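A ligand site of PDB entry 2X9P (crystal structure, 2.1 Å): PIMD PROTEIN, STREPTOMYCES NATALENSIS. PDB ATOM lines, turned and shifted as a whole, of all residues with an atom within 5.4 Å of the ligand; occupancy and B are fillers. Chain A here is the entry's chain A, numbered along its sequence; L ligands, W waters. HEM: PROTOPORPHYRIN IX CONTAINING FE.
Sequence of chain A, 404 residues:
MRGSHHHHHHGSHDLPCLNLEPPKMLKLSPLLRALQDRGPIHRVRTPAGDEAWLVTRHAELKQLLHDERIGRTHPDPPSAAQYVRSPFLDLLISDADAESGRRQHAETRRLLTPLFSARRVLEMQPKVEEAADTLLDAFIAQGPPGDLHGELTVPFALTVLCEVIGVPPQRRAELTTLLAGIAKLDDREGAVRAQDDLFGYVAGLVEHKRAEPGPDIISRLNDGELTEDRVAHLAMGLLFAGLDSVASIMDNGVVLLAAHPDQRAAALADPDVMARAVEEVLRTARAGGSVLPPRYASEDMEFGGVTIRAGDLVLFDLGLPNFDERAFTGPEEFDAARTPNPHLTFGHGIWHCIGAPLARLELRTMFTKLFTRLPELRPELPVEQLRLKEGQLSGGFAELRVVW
N of Gly 355 lies close to SG of Cys 353 (3.4 Å).
N of Cys 353 is in hydrogen-bond range of O of Phe 346, 2.8 Å away.
The side-chain sulfur of Cys 353 sits close to the backbone NH of Ala 356 (3.3 Å).
The guanidinium group of Arg 109 sits at hydrogen-bond distance from the backbone carbonyl oxygen of Ile 350 (3.4 Å).
The backbone carbonyl oxygen (O) of His 352 lies within hydrogen-bond range of the guanidinium group (NH1) of Arg 109 (2.9 Å).
The backbone carbonyl oxygen (O) of Ile 350 sits close to a ring nitrogen (NE2) of His 105 (3.4 Å).
The guanidinium group of Arg 295 is in hydrogen-bond range of the backbone carbonyl oxygen of Pro 293 (2.8 Å).
The side-chain hydroxyl (OG) of Ser 245 lies within hydrogen-bond range of the backbone carbonyl oxygen (O) of Ala 241, 2.7 Å away.
An iron atom (FE) of the ligand is bound by the side-chain sulfur of Cys 353 (2.3 Å).
NH1 of Arg 109 lies within salt-bridge range of O1D of the ligand (2.5 Å).
A ring nitrogen (NE2) of His 105 sits at hydrogen-bond distance from an oxygen (O1D) of the ligand, 2.7 Å away.
NH1 of Arg 295 lies within salt-bridge range of O2A of the ligand, 2.8 Å away.
O2A of the ligand is in salt-bridge range of NH2 of Arg 72, at 3.6 Å.
O of Ile 350 sits close to O1D of the ligand, 3.2 Å away.
Merely in contact with the ligand: Trp 351, Val 246, Ser 245, Pro 293, Gly 355, Leu 161, Leu 318, Thr 345, Ala 241, Gly 242, Phe 346, Leu 292, Leu 112, Gly 347, Ala 359, Phe 116, His 352, Leu 238, Ile 354 and Glu 362.
Hydrophobic or aromatic side chains within 4 Å of the ligand: His 105, Leu 112, Phe 116, Leu 161, Leu 238, Ala 241, Val 246, Leu 292, Pro 293, Leu 318, Phe 346, Trp 351, Ile 354 and Ala 359.
Within 4 Å of the ligand: Arg 72, His 105, Arg 109, Leu 112, Phe 116, Leu 161, Leu 238, Ala 241, Gly 242, Ser 245, Val 246, Leu 292, Pro 293, Arg 295, Leu 318, Thr 345, Phe 346, Gly 347, Ile 350, Trp 351, His 352, Cys 353, Ile 354, Gly 355, Ala 359 and Glu 362.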
ATOM      1  N   ARG A  72     -12.096  14.220 -22.858  1.00  0.00           N
ATOM      2  CA  ARG A  72     -11.382  13.760 -21.659  1.00  0.00           C
ATOM      3  C   ARG A  72     -10.656  12.452 -21.857  1.00  0.00           C
ATOM      4  O   ARG A  72     -10.200  11.845 -20.858  1.00  0.00           O
ATOM      5  CB  ARG A  72     -12.349  13.528 -20.494  1.00  0.00           C
ATOM      6  CG  ARG A  72     -13.158  14.744 -20.154  1.00  0.00           C
ATOM      7  CD  ARG A  72     -13.915  14.444 -18.827  1.00  0.00           C
ATOM      8  NE  ARG A  72     -14.852  15.525 -18.500  1.00  0.00           N
ATOM      9  CZ  ARG A  72     -14.524  16.609 -17.786  1.00  0.00           C
ATOM     10  NH1 ARG A  72     -13.290  16.743 -17.310  1.00  0.00           N
ATOM     11  NH2 ARG A  72     -15.464  17.537 -17.535  1.00  0.00           N
ATOM     12  N   HIS A 105     -20.270  11.259 -22.332  1.00  0.00           N
ATOM     13  CA  HIS A 105     -20.528  12.676 -22.109  1.00  0.00           C
ATOM     14  C   HIS A 105     -21.918  13.103 -22.595  1.00  0.00           C
ATOM     15  O   HIS A 105     -22.693  13.660 -21.791  1.00  0.00           O
ATOM     16  CB  HIS A 105     -19.431  13.523 -22.710  1.00  0.00           C
ATOM     17  CG  HIS A 105     -19.549  14.979 -22.364  1.00  0.00           C
ATOM     18  ND1 HIS A 105     -19.172  15.969 -23.237  1.00  0.00           N
ATOM     19  CD2 HIS A 105     -19.996  15.597 -21.246  1.00  0.00           C
ATOM     20  CE1 HIS A 105     -19.390  17.143 -22.667  1.00  0.00           C
ATOM     21  NE2 HIS A 105     -19.925  16.939 -21.472  1.00  0.00           N
ATOM     22  N   ARG A 109     -25.147  14.522 -20.199  1.00  0.00           N
ATOM     23  CA  ARG A 109     -25.873  15.804 -20.476  1.00  0.00           C
ATOM     24  C   ARG A 109     -27.368  15.611 -20.698  1.00  0.00           C
ATOM     25  O   ARG A 109     -28.165  16.348 -20.136  1.00  0.00           O
ATOM     26  CB  ARG A 109     -25.258  16.613 -21.627  1.00  0.00           C
ATOM     27  CG  ARG A 109     -23.769  16.974 -21.383  1.00  0.00           C
ATOM     28  CD  ARG A 109     -23.289  17.953 -22.465  1.00  0.00           C
ATOM     29  NE  ARG A 109     -24.169  19.161 -22.562  1.00  0.00           N
ATOM     30  CZ  ARG A 109     -24.000  20.288 -21.819  1.00  0.00           C
ATOM     31  NH1 ARG A 109     -23.039  20.382 -20.889  1.00  0.00           N
ATOM     32  NH2 ARG A 109     -24.822  21.338 -21.975  1.00  0.00           N
ATOM     33  N   LEU A 112     -28.959  14.915 -17.244  1.00  0.00           N
ATOM     34  CA  LEU A 112     -28.887  15.942 -16.211  1.00  0.00           C
ATOM     35  C   LEU A 112     -29.700  17.180 -16.600  1.00  0.00           C
ATOM     36  O   LEU A 112     -30.299  17.794 -15.743  1.00  0.00           O
ATOM     37  CB  LEU A 112     -27.416  16.283 -15.872  1.00  0.00           C
ATOM     38  CG  LEU A 112     -26.564  15.202 -15.188  1.00  0.00           C
ATOM     39  CD1 LEU A 112     -25.203  15.759 -14.845  1.00  0.00           C
ATOM     40  CD2 LEU A 112     -27.253  14.871 -13.878  1.00  0.00           C
ATOM     41  N   PHE A 116     -32.817  20.495 -14.538  1.00  0.00           N
ATOM     42  CA  PHE A 116     -32.609  21.923 -14.324  1.00  0.00           C
ATOM     43  C   PHE A 116     -33.467  22.716 -15.302  1.00  0.00           C
ATOM     44  O   PHE A 116     -33.086  23.780 -15.681  1.00  0.00           O
ATOM     45  CB  PHE A 116     -31.104  22.299 -14.480  1.00  0.00           C
ATOM     46  CG  PHE A 116     -30.241  21.751 -13.357  1.00  0.00           C
ATOM     47  CD1 PHE A 116     -30.071  22.498 -12.196  1.00  0.00           C
ATOM     48  CD2 PHE A 116     -29.669  20.475 -13.426  1.00  0.00           C
ATOM     49  CE1 PHE A 116     -29.300  22.018 -11.104  1.00  0.00           C
ATOM     50  CE2 PHE A 116     -28.947  19.945 -12.324  1.00  0.00           C
ATOM     51  CZ  PHE A 116     -28.745  20.730 -11.151  1.00  0.00           C
ATOM     52  N   LEU A 161     -27.054  22.315  -2.261  1.00  0.00           N
ATOM     53  CA  LEU A 161     -26.853  21.009  -2.901  1.00  0.00           C
ATOM     54  C   LEU A 161     -27.607  19.891  -2.175  1.00  0.00           C
ATOM     55  O   LEU A 161     -28.319  19.099  -2.823  1.00  0.00           O
ATOM     56  CB  LEU A 161     -25.350  20.630  -3.062  1.00  0.00           C
ATOM     57  CG  LEU A 161     -24.561  21.314  -4.152  1.00  0.00           C
ATOM     58  CD1 LEU A 161     -23.001  21.068  -3.996  1.00  0.00           C
ATOM     59  CD2 LEU A 161     -25.032  20.820  -5.558  1.00  0.00           C
ATOM     60  N   LEU A 238     -22.608  15.929  -9.267  1.00  0.00           N
ATOM     61  CA  LEU A 238     -23.287  17.193  -8.968  1.00  0.00           C
ATOM     62  C   LEU A 238     -22.704  17.862  -7.715  1.00  0.00           C
ATOM     63  O   LEU A 238     -22.445  19.098  -7.701  1.00  0.00           O
ATOM     64  CB  LEU A 238     -24.781  16.989  -8.815  1.00  0.00           C
ATOM     65  CG  LEU A 238     -25.510  16.767 -10.131  1.00  0.00           C
ATOM     66  CD1 LEU A 238     -26.893  16.218  -9.918  1.00  0.00           C
ATOM     67  CD2 LEU A 238     -25.511  18.075 -11.088  1.00  0.00           C
ATOM     68  N   ALA A 241     -19.518  19.468  -8.878  1.00  0.00           N
ATOM     69  CA  ALA A 241     -19.695  20.594  -9.765  1.00  0.00           C
ATOM     70  C   ALA A 241     -20.250  21.815  -9.045  1.00  0.00           C
ATOM     71  O   ALA A 241     -19.975  22.928  -9.455  1.00  0.00           O
ATOM     72  CB  ALA A 241     -20.672  20.190 -10.889  1.00  0.00           C
ATOM     73  N   GLY A 242     -21.074  21.611  -7.998  1.00  0.00           N
ATOM     74  CA  GLY A 242     -21.871  22.715  -7.478  1.00  0.00           C
ATOM     75  C   GLY A 242     -21.401  23.356  -6.207  1.00  0.00           C
ATOM     76  O   GLY A 242     -22.054  24.283  -5.700  1.00  0.00           O
ATOM     77  N   SER A 245     -17.257  25.833  -6.802  1.00  0.00           N
ATOM     78  CA  SER A 245     -17.529  26.818  -7.826  1.00  0.00           C
ATOM     79  C   SER A 245     -18.408  27.921  -7.276  1.00  0.00           C
ATOM     80  O   SER A 245     -18.090  29.090  -7.397  1.00  0.00           O
ATOM     81  CB  SER A 245     -18.224  26.128  -9.024  1.00  0.00           C
ATOM     82  OG  SER A 245     -19.438  25.447  -8.598  1.00  0.00           O
ATOM     83  N   VAL A 246     -19.550  27.567  -6.737  1.00  0.00           N
ATOM     84  CA  VAL A 246     -20.458  28.570  -6.179  1.00  0.00           C
ATOM     85  C   VAL A 246     -19.764  29.412  -5.078  1.00  0.00           C
ATOM     86  O   VAL A 246     -19.726  30.675  -5.128  1.00  0.00           O
ATOM     87  CB  VAL A 246     -21.780  27.902  -5.645  1.00  0.00           C
ATOM     88  CG1 VAL A 246     -22.686  28.950  -4.864  1.00  0.00           C
ATOM     89  CG2 VAL A 246     -22.549  27.274  -6.828  1.00  0.00           C
ATOM     90  N   ALA A 247     -19.140  28.723  -4.129  1.00  0.00           N
ATOM     91  CA  ALA A 247     -18.522  29.434  -2.994  1.00  0.00           C
ATOM     92  C   ALA A 247     -17.468  30.382  -3.494  1.00  0.00           C
ATOM     93  O   ALA A 247     -17.294  31.494  -2.978  1.00  0.00           O
ATOM     94  CB  ALA A 247     -17.888  28.416  -1.993  1.00  0.00           C
ATOM     95  N   ILE A 249     -17.086  31.869  -6.613  1.00  0.00           N
ATOM     96  CA  ILE A 249     -17.645  33.047  -7.283  1.00  0.00           C
ATOM     97  C   ILE A 249     -18.303  33.981  -6.208  1.00  0.00           C
ATOM     98  O   ILE A 249     -18.187  35.231  -6.267  1.00  0.00           O
ATOM     99  CB  ILE A 249     -18.675  32.622  -8.384  1.00  0.00           C
ATOM    100  CG1 ILE A 249     -17.977  31.804  -9.517  1.00  0.00           C
ATOM    101  CG2 ILE A 249     -19.426  33.825  -8.927  1.00  0.00           C
ATOM    102  CD1 ILE A 249     -16.823  32.524 -10.260  1.00  0.00           C
ATOM    103  N   LEU A 282     -19.633  37.104 -12.345  1.00  0.00           N
ATOM    104  CA  LEU A 282     -19.201  35.873 -13.028  1.00  0.00           C
ATOM    105  C   LEU A 282     -18.095  36.173 -14.045  1.00  0.00           C
ATOM    106  O   LEU A 282     -17.106  35.421 -14.102  1.00  0.00           O
ATOM    107  CB  LEU A 282     -20.375  35.187 -13.727  1.00  0.00           C
ATOM    108  CG  LEU A 282     -21.307  34.518 -12.709  1.00  0.00           C
ATOM    109  CD1 LEU A 282     -22.726  34.407 -13.320  1.00  0.00           C
ATOM    110  CD2 LEU A 282     -20.793  33.032 -12.423  1.00  0.00           C
ATOM    111  N   ARG A 286     -12.375  35.858 -11.679  1.00  0.00           N
ATOM    112  CA  ARG A 286     -10.940  35.514 -11.859  1.00  0.00           C
ATOM    113  C   ARG A 286     -10.341  36.014 -13.204  1.00  0.00           C
ATOM    114  O   ARG A 286     -10.742  35.576 -14.253  1.00  0.00           O
ATOM    115  CB  ARG A 286     -10.716  33.982 -11.762  1.00  0.00           C
ATOM    116  CG  ARG A 286     -11.270  33.278 -10.502  1.00  0.00           C
ATOM    117  CD  ARG A 286     -12.318  32.260 -11.070  1.00  0.00           C
ATOM    118  NE  ARG A 286     -12.626  31.127 -10.199  1.00  0.00           N
ATOM    119  CZ  ARG A 286     -13.533  30.178 -10.460  1.00  0.00           C
ATOM    120  NH1 ARG A 286     -13.729  29.201  -9.585  1.00  0.00           N
ATOM    121  NH2 ARG A 286     -14.257  30.198 -11.595  1.00  0.00           N
ATOM    122  N   LEU A 292      -9.822  25.141 -16.654  1.00  0.00           N
ATOM    123  CA  LEU A 292     -10.656  23.918 -16.476  1.00  0.00           C
ATOM    124  C   LEU A 292      -9.752  22.641 -16.392  1.00  0.00           C
ATOM    125  O   LEU A 292      -8.524  22.752 -16.687  1.00  0.00           O
ATOM    126  CB  LEU A 292     -11.676  23.807 -17.592  1.00  0.00           C
ATOM    127  CG  LEU A 292     -12.542  25.063 -17.591  1.00  0.00           C
ATOM    128  CD1 LEU A 292     -13.538  24.858 -18.687  1.00  0.00           C
ATOM    129  CD2 LEU A 292     -13.177  25.282 -16.173  1.00  0.00           C
ATOM    130  N   PRO A 293     -10.326  21.478 -15.960  1.00  0.00           N
ATOM    131  CA  PRO A 293      -9.639  20.178 -15.953  1.00  0.00           C
ATOM    132  C   PRO A 293      -9.132  19.770 -17.340  1.00  0.00           C
ATOM    133  O   PRO A 293      -9.654  20.248 -18.334  1.00  0.00           O
ATOM    134  CB  PRO A 293     -10.744  19.196 -15.491  1.00  0.00           C
ATOM    135  CG  PRO A 293     -11.496  20.073 -14.413  1.00  0.00           C
ATOM    136  CD  PRO A 293     -11.581  21.419 -15.146  1.00  0.00           C
ATOM    137  N   ARG A 295      -8.111  18.601 -21.000  1.00  0.00           N
ATOM    138  CA  ARG A 295      -8.841  18.185 -22.115  1.00  0.00           C
ATOM    139  C   ARG A 295      -7.876  17.994 -23.280  1.00  0.00           C
ATOM    140  O   ARG A 295      -6.896  18.751 -23.398  1.00  0.00           O
ATOM    141  CB  ARG A 295      -9.820  19.272 -22.447  1.00  0.00           C
ATOM    142  CG  ARG A 295     -11.082  18.676 -22.835  1.00  0.00           C
ATOM    143  CD  ARG A 295     -12.135  18.760 -21.847  1.00  0.00           C
ATOM    144  NE  ARG A 295     -11.786  19.112 -20.464  1.00  0.00           N
ATOM    145  CZ  ARG A 295     -12.686  19.750 -19.713  1.00  0.00           C
ATOM    146  NH1 ARG A 295     -13.841  20.076 -20.278  1.00  0.00           N
ATOM    147  NH2 ARG A 295     -12.409  20.091 -18.477  1.00  0.00           N
ATOM    148  N   LEU A 318     -10.928  30.326 -18.861  1.00  0.00           N
ATOM    149  CA  LEU A 318     -12.129  31.080 -19.191  1.00  0.00           C
ATOM    150  C   LEU A 318     -11.910  32.554 -18.858  1.00  0.00           C
ATOM    151  O   LEU A 318     -12.550  33.416 -19.463  1.00  0.00           O
ATOM    152  CB  LEU A 318     -13.330  30.531 -18.419  1.00  0.00           C
ATOM    153  CG  LEU A 318     -13.686  29.104 -18.757  1.00  0.00           C
ATOM    154  CD1 LEU A 318     -14.867  28.505 -17.914  1.00  0.00           C
ATOM    155  CD2 LEU A 318     -14.004  28.920 -20.299  1.00  0.00           C
ATOM    156  N   LEU A 344     -17.936  33.710 -20.438  1.00  0.00           N
ATOM    157  CA  LEU A 344     -17.879  32.265 -20.691  1.00  0.00           C
ATOM    158  C   LEU A 344     -17.632  31.558 -19.345  1.00  0.00           C
ATOM    159  O   LEU A 344     -17.105  30.462 -19.297  1.00  0.00           O
ATOM    160  CB  LEU A 344     -16.740  31.927 -21.691  1.00  0.00           C
ATOM    161  CG  LEU A 344     -16.945  32.529 -23.101  1.00  0.00           C
ATOM    162  CD1 LEU A 344     -15.837  32.047 -24.061  1.00  0.00           C
ATOM    163  CD2 LEU A 344     -18.338  32.093 -23.699  1.00  0.00           C
ATOM    164  N   THR A 345     -18.047  32.197 -18.252  1.00  0.00           N
ATOM    165  CA  THR A 345     -17.767  31.611 -16.934  1.00  0.00           C
ATOM    166  C   THR A 345     -18.513  30.308 -16.704  1.00  0.00           C
ATOM    167  O   THR A 345     -18.039  29.487 -15.952  1.00  0.00           O
ATOM    168  CB  THR A 345     -17.990  32.643 -15.823  1.00  0.00           C
ATOM    169  OG1 THR A 345     -17.089  33.732 -16.088  1.00  0.00           O
ATOM    170  CG2 THR A 345     -17.621  32.075 -14.419  1.00  0.00           C
ATOM    171  N   PHE A 346     -19.665  30.129 -17.345  1.00  0.00           N
ATOM    172  CA  PHE A 346     -20.344  28.830 -17.359  1.00  0.00           C
ATOM    173  C   PHE A 346     -19.914  27.892 -18.492  1.00  0.00           C
ATOM    174  O   PHE A 346     -20.650  26.957 -18.842  1.00  0.00           O
ATOM    175  CB  PHE A 346     -21.878  29.039 -17.380  1.00  0.00           C
ATOM    176  CG  PHE A 346     -22.403  29.540 -16.094  1.00  0.00           C
ATOM    177  CD1 PHE A 346     -22.198  28.800 -14.889  1.00  0.00           C
ATOM    178  CD2 PHE A 346     -23.091  30.761 -16.023  1.00  0.00           C
ATOM    179  CE1 PHE A 346     -22.736  29.238 -13.666  1.00  0.00           C
ATOM    180  CE2 PHE A 346     -23.605  31.233 -14.757  1.00  0.00           C
ATOM    181  CZ  PHE A 346     -23.441  30.461 -13.607  1.00  0.00           C
ATOM    182  N   GLY A 347     -18.735  28.131 -19.088  1.00  0.00           N
ATOM    183  CA  GLY A 347     -18.359  27.361 -20.255  1.00  0.00           C
ATOM    184  C   GLY A 347     -19.229  27.673 -21.427  1.00  0.00           C
ATOM    185  O   GLY A 347     -19.863  28.778 -21.512  1.00  0.00           O
ATOM    186  N   ILE A 350     -20.242  22.204 -25.744  1.00  0.00           N
ATOM    187  CA  ILE A 350     -20.380  20.868 -25.199  1.00  0.00           C
ATOM    188  C   ILE A 350     -20.044  20.807 -23.726  1.00  0.00           C
ATOM    189  O   ILE A 350     -20.457  19.887 -23.005  1.00  0.00           O
ATOM    190  CB  ILE A 350     -19.641  19.734 -26.052  1.00  0.00           C
ATOM    191  CG1 ILE A 350     -18.094  19.874 -26.006  1.00  0.00           C
ATOM    192  CG2 ILE A 350     -20.202  19.721 -27.490  1.00  0.00           C
ATOM    193  CD1 ILE A 350     -17.381  19.050 -27.179  1.00  0.00           C
ATOM    194  N   TRP A 351     -19.308  21.812 -23.273  1.00  0.00           N
ATOM    195  CA  TRP A 351     -18.909  21.930 -21.900  1.00  0.00           C
ATOM    196  C   TRP A 351     -19.794  22.954 -21.083  1.00  0.00           C
ATOM    197  O   TRP A 351     -19.378  23.434 -20.067  1.00  0.00           O
ATOM    198  CB  TRP A 351     -17.409  22.259 -21.821  1.00  0.00           C
ATOM    199  CG  TRP A 351     -16.551  21.312 -22.675  1.00  0.00           C
ATOM    200  CD1 TRP A 351     -15.842  21.605 -23.841  1.00  0.00           C
ATOM    201  CD2 TRP A 351     -16.339  19.895 -22.431  1.00  0.00           C
ATOM    202  NE1 TRP A 351     -15.185  20.461 -24.302  1.00  0.00           N
ATOM    203  CE2 TRP A 351     -15.479  19.403 -23.476  1.00  0.00           C
ATOM    204  CE3 TRP A 351     -16.725  19.029 -21.397  1.00  0.00           C
ATOM    205  CZ2 TRP A 351     -15.066  18.042 -23.540  1.00  0.00           C
ATOM    206  CZ3 TRP A 351     -16.302  17.655 -21.443  1.00  0.00           C
ATOM    207  CH2 TRP A 351     -15.462  17.198 -22.523  1.00  0.00           C
ATOM    208  N   HIS A 352     -21.010  23.242 -21.474  1.00  0.00           N
ATOM    209  CA  HIS A 352     -21.744  24.298 -20.733  1.00  0.00           C
ATOM    210  C   HIS A 352     -22.304  23.820 -19.335  1.00  0.00           C
ATOM    211  O   HIS A 352     -22.872  22.758 -19.254  1.00  0.00           O
ATOM    212  CB  HIS A 352     -22.917  24.819 -21.597  1.00  0.00           C
ATOM    213  CG  HIS A 352     -23.662  25.947 -20.954  1.00  0.00           C
ATOM    214  ND1 HIS A 352     -24.904  25.786 -20.394  1.00  0.00           N
ATOM    215  CD2 HIS A 352     -23.304  27.236 -20.734  1.00  0.00           C
ATOM    216  CE1 HIS A 352     -25.294  26.931 -19.860  1.00  0.00           C
ATOM    217  NE2 HIS A 352     -24.349  27.830 -20.062  1.00  0.00           N
ATOM    218  N   CYS A 353     -22.155  24.642 -18.291  1.00  0.00           N
ATOM    219  CA  CYS A 353     -22.660  24.341 -16.962  1.00  0.00           C
ATOM    220  C   CYS A 353     -24.167  24.015 -16.973  1.00  0.00           C
ATOM    221  O   CYS A 353     -24.997  24.899 -17.257  1.00  0.00           O
ATOM    222  CB  CYS A 353     -22.375  25.539 -16.000  1.00  0.00           C
ATOM    223  SG  CYS A 353     -23.004  25.140 -14.376  1.00  0.00           S
ATOM    224  N   ILE A 354     -24.517  22.777 -16.673  1.00  0.00           N
ATOM    225  CA  ILE A 354     -25.934  22.384 -16.579  1.00  0.00           C
ATOM    226  C   ILE A 354     -26.626  22.986 -15.314  1.00  0.00           C
ATOM    227  O   ILE A 354     -27.862  23.231 -15.322  1.00  0.00           O
ATOM    228  CB  ILE A 354     -26.051  20.825 -16.645  1.00  0.00           C
ATOM    229  CG1 ILE A 354     -25.603  20.343 -18.067  1.00  0.00           C
ATOM    230  CG2 ILE A 354     -27.477  20.307 -16.326  1.00  0.00           C
ATOM    231  CD1 ILE A 354     -25.678  18.804 -18.320  1.00  0.00           C
ATOM    232  N   GLY A 355     -25.841  23.246 -14.273  1.00  0.00           N
ATOM    233  CA  GLY A 355     -26.386  23.905 -13.036  1.00  0.00           C
ATOM    234  C   GLY A 355     -26.517  25.418 -13.095  1.00  0.00           C
ATOM    235  O   GLY A 355     -26.936  26.027 -12.091  1.00  0.00           O
ATOM    236  N   ALA A 356     -26.186  26.027 -14.237  1.00  0.00           N
ATOM    237  CA  ALA A 356     -26.103  27.486 -14.336  1.00  0.00           C
ATOM    238  C   ALA A 356     -27.336  28.223 -13.792  1.00  0.00           C
ATOM    239  O   ALA A 356     -27.137  29.154 -13.020  1.00  0.00           O
ATOM    240  CB  ALA A 356     -25.767  27.977 -15.776  1.00  0.00           C
ATOM    241  N   LEU A 358     -29.409  27.363 -11.468  1.00  0.00           N
ATOM    242  CA  LEU A 358     -29.292  27.252 -10.003  1.00  0.00           C
ATOM    243  C   LEU A 358     -28.139  28.087  -9.462  1.00  0.00           C
ATOM    244  O   LEU A 358     -28.279  28.793  -8.443  1.00  0.00           O
ATOM    245  CB  LEU A 358     -29.089  25.790  -9.539  1.00  0.00           C
ATOM    246  CG  LEU A 358     -28.949  25.570  -8.019  1.00  0.00           C
ATOM    247  CD1 LEU A 358     -30.184  26.208  -7.218  1.00  0.00           C
ATOM    248  CD2 LEU A 358     -28.868  24.015  -7.658  1.00  0.00           C
ATOM    249  N   ALA A 359     -26.993  28.012 -10.120  1.00  0.00           N
ATOM    250  CA  ALA A 359     -25.910  28.827  -9.641  1.00  0.00           C
ATOM    251  C   ALA A 359     -26.302  30.344  -9.634  1.00  0.00           C
ATOM    252  O   ALA A 359     -26.013  31.059  -8.674  1.00  0.00           O
ATOM    253  CB  ALA A 359     -24.582  28.590 -10.454  1.00  0.00           C
ATOM    254  N   GLU A 362     -28.443  31.099  -6.687  1.00  0.00           N
ATOM    255  CA  GLU A 362     -27.688  31.223  -5.410  1.00  0.00           C
ATOM    256  C   GLU A 362     -26.941  32.514  -5.265  1.00  0.00           C
ATOM    257  O   GLU A 362     -26.926  33.146  -4.183  1.00  0.00           O
ATOM    258  CB  GLU A 362     -26.697  30.078  -5.196  1.00  0.00           C
ATOM    259  CG  GLU A 362     -27.358  28.685  -5.181  1.00  0.00           C
ATOM    260  CD  GLU A 362     -26.358  27.582  -4.812  1.00  0.00           C
ATOM    261  OE1 GLU A 362     -25.680  27.759  -3.789  1.00  0.00           O
ATOM    262  OE2 GLU A 362     -26.212  26.605  -5.583  1.00  0.00           O
ATOM    263  N   LEU A 363     -26.299  32.942  -6.344  1.00  0.00           N
ATOM    264  CA  LEU A 363     -25.597  34.198  -6.319  1.00  0.00           C
ATOM    265  C   LEU A 363     -26.574  35.419  -6.141  1.00  0.00           C
ATOM    266  O   LEU A 363     -26.330  36.260  -5.310  1.00  0.00           O
ATOM    267  CB  LEU A 363     -24.751  34.376  -7.583  1.00  0.00           C
ATOM    268  CG  LEU A 363     -23.613  33.356  -7.731  1.00  0.00           C
ATOM    269  CD1 LEU A 363     -23.193  33.358  -9.240  1.00  0.00           C
ATOM    270  CD2 LEU A 363     -22.459  33.606  -6.645  1.00  0.00           C
HETATM  271  CHA HEM L   1     -19.970  22.090 -15.817  1.00  0.00           C
HETATM  272  CHB HEM L   1     -18.965  26.483 -14.168  1.00  0.00           C
HETATM  273  CHC HEM L   1     -22.120  25.705 -10.561  1.00  0.00           C
HETATM  274  CHD HEM L   1     -23.492  21.573 -12.499  1.00  0.00           C
HETATM  275  C1A HEM L   1     -19.430  23.328 -15.661  1.00  0.00           C
HETATM  276  C2A HEM L   1     -18.411  23.906 -16.518  1.00  0.00           C
HETATM  277  C3A HEM L   1     -18.098  25.128 -16.045  1.00  0.00           C
HETATM  278  C4A HEM L   1     -18.978  25.361 -14.927  1.00  0.00           C
HETATM  279  CMA HEM L   1     -17.079  26.159 -16.550  1.00  0.00           C
HETATM  280  CAA HEM L   1     -17.702  23.126 -17.642  1.00  0.00           C
HETATM  281  CBA HEM L   1     -16.576  22.534 -16.755  1.00  0.00           C
HETATM  282  CGA HEM L   1     -15.560  21.645 -17.472  1.00  0.00           C
HETATM  283  O1A HEM L   1     -14.396  21.577 -16.964  1.00  0.00           O
HETATM  284  O2A HEM L   1     -15.854  20.989 -18.504  1.00  0.00           O
HETATM  285  C1B HEM L   1     -19.755  26.628 -13.020  1.00  0.00           C
HETATM  286  C2B HEM L   1     -19.783  27.838 -12.222  1.00  0.00           C
HETATM  287  C3B HEM L   1     -20.642  27.644 -11.246  1.00  0.00           C
HETATM  288  C4B HEM L   1     -21.180  26.293 -11.388  1.00  0.00           C
HETATM  289  CMB HEM L   1     -19.003  29.138 -12.430  1.00  0.00           C
HETATM  290  CAB HEM L   1     -20.938  28.839 -10.304  1.00  0.00           C
HETATM  291  CBB HEM L   1     -21.130  28.602  -9.121  1.00  0.00           C
HETATM  292  C1C HEM L   1     -22.817  24.549 -10.757  1.00  0.00           C
HETATM  293  C2C HEM L   1     -23.966  24.057  -9.980  1.00  0.00           C
HETATM  294  C3C HEM L   1     -24.295  22.892 -10.508  1.00  0.00           C
HETATM  295  C4C HEM L   1     -23.412  22.651 -11.650  1.00  0.00           C
HETATM  296  CMC HEM L   1     -24.603  24.760  -8.742  1.00  0.00           C
HETATM  297  CAC HEM L   1     -25.430  21.915 -10.163  1.00  0.00           C
HETATM  298  CBC HEM L   1     -25.706  21.610  -8.885  1.00  0.00           C
HETATM  299  C1D HEM L   1     -22.676  21.358 -13.574  1.00  0.00           C
HETATM  300  C2D HEM L   1     -22.703  20.149 -14.361  1.00  0.00           C
HETATM  301  C3D HEM L   1     -21.617  20.268 -15.382  1.00  0.00           C
HETATM  302  C4D HEM L   1     -21.001  21.559 -15.096  1.00  0.00           C
HETATM  303  CMD HEM L   1     -23.625  18.941 -14.194  1.00  0.00           C
HETATM  304  CAD HEM L   1     -21.267  19.153 -16.427  1.00  0.00           C
HETATM  305  CBD HEM L   1     -21.741  19.555 -17.831  1.00  0.00           C
HETATM  306  CGD HEM L   1     -20.881  18.928 -18.936  1.00  0.00           C
HETATM  307  O1D HEM L   1     -21.332  18.797 -20.091  1.00  0.00           O
HETATM  308  O2D HEM L   1     -19.716  18.547 -18.684  1.00  0.00           O
HETATM  309  NA  HEM L   1     -19.780  24.252 -14.705  1.00  0.00           N
HETATM  310  NB  HEM L   1     -20.638  25.711 -12.498  1.00  0.00           N
HETATM  311  NC  HEM L   1     -22.535  23.655 -11.769  1.00  0.00           N
HETATM  312  ND  HEM L   1     -21.666  22.182 -14.030  1.00  0.00           N
HETATM  313 FE   HEM L   1     -21.290  23.990 -13.330  1.00  0.00          FE
HETATM  314  O   HOH W   1     -19.128  23.198 -12.058  1.00  0.00           O
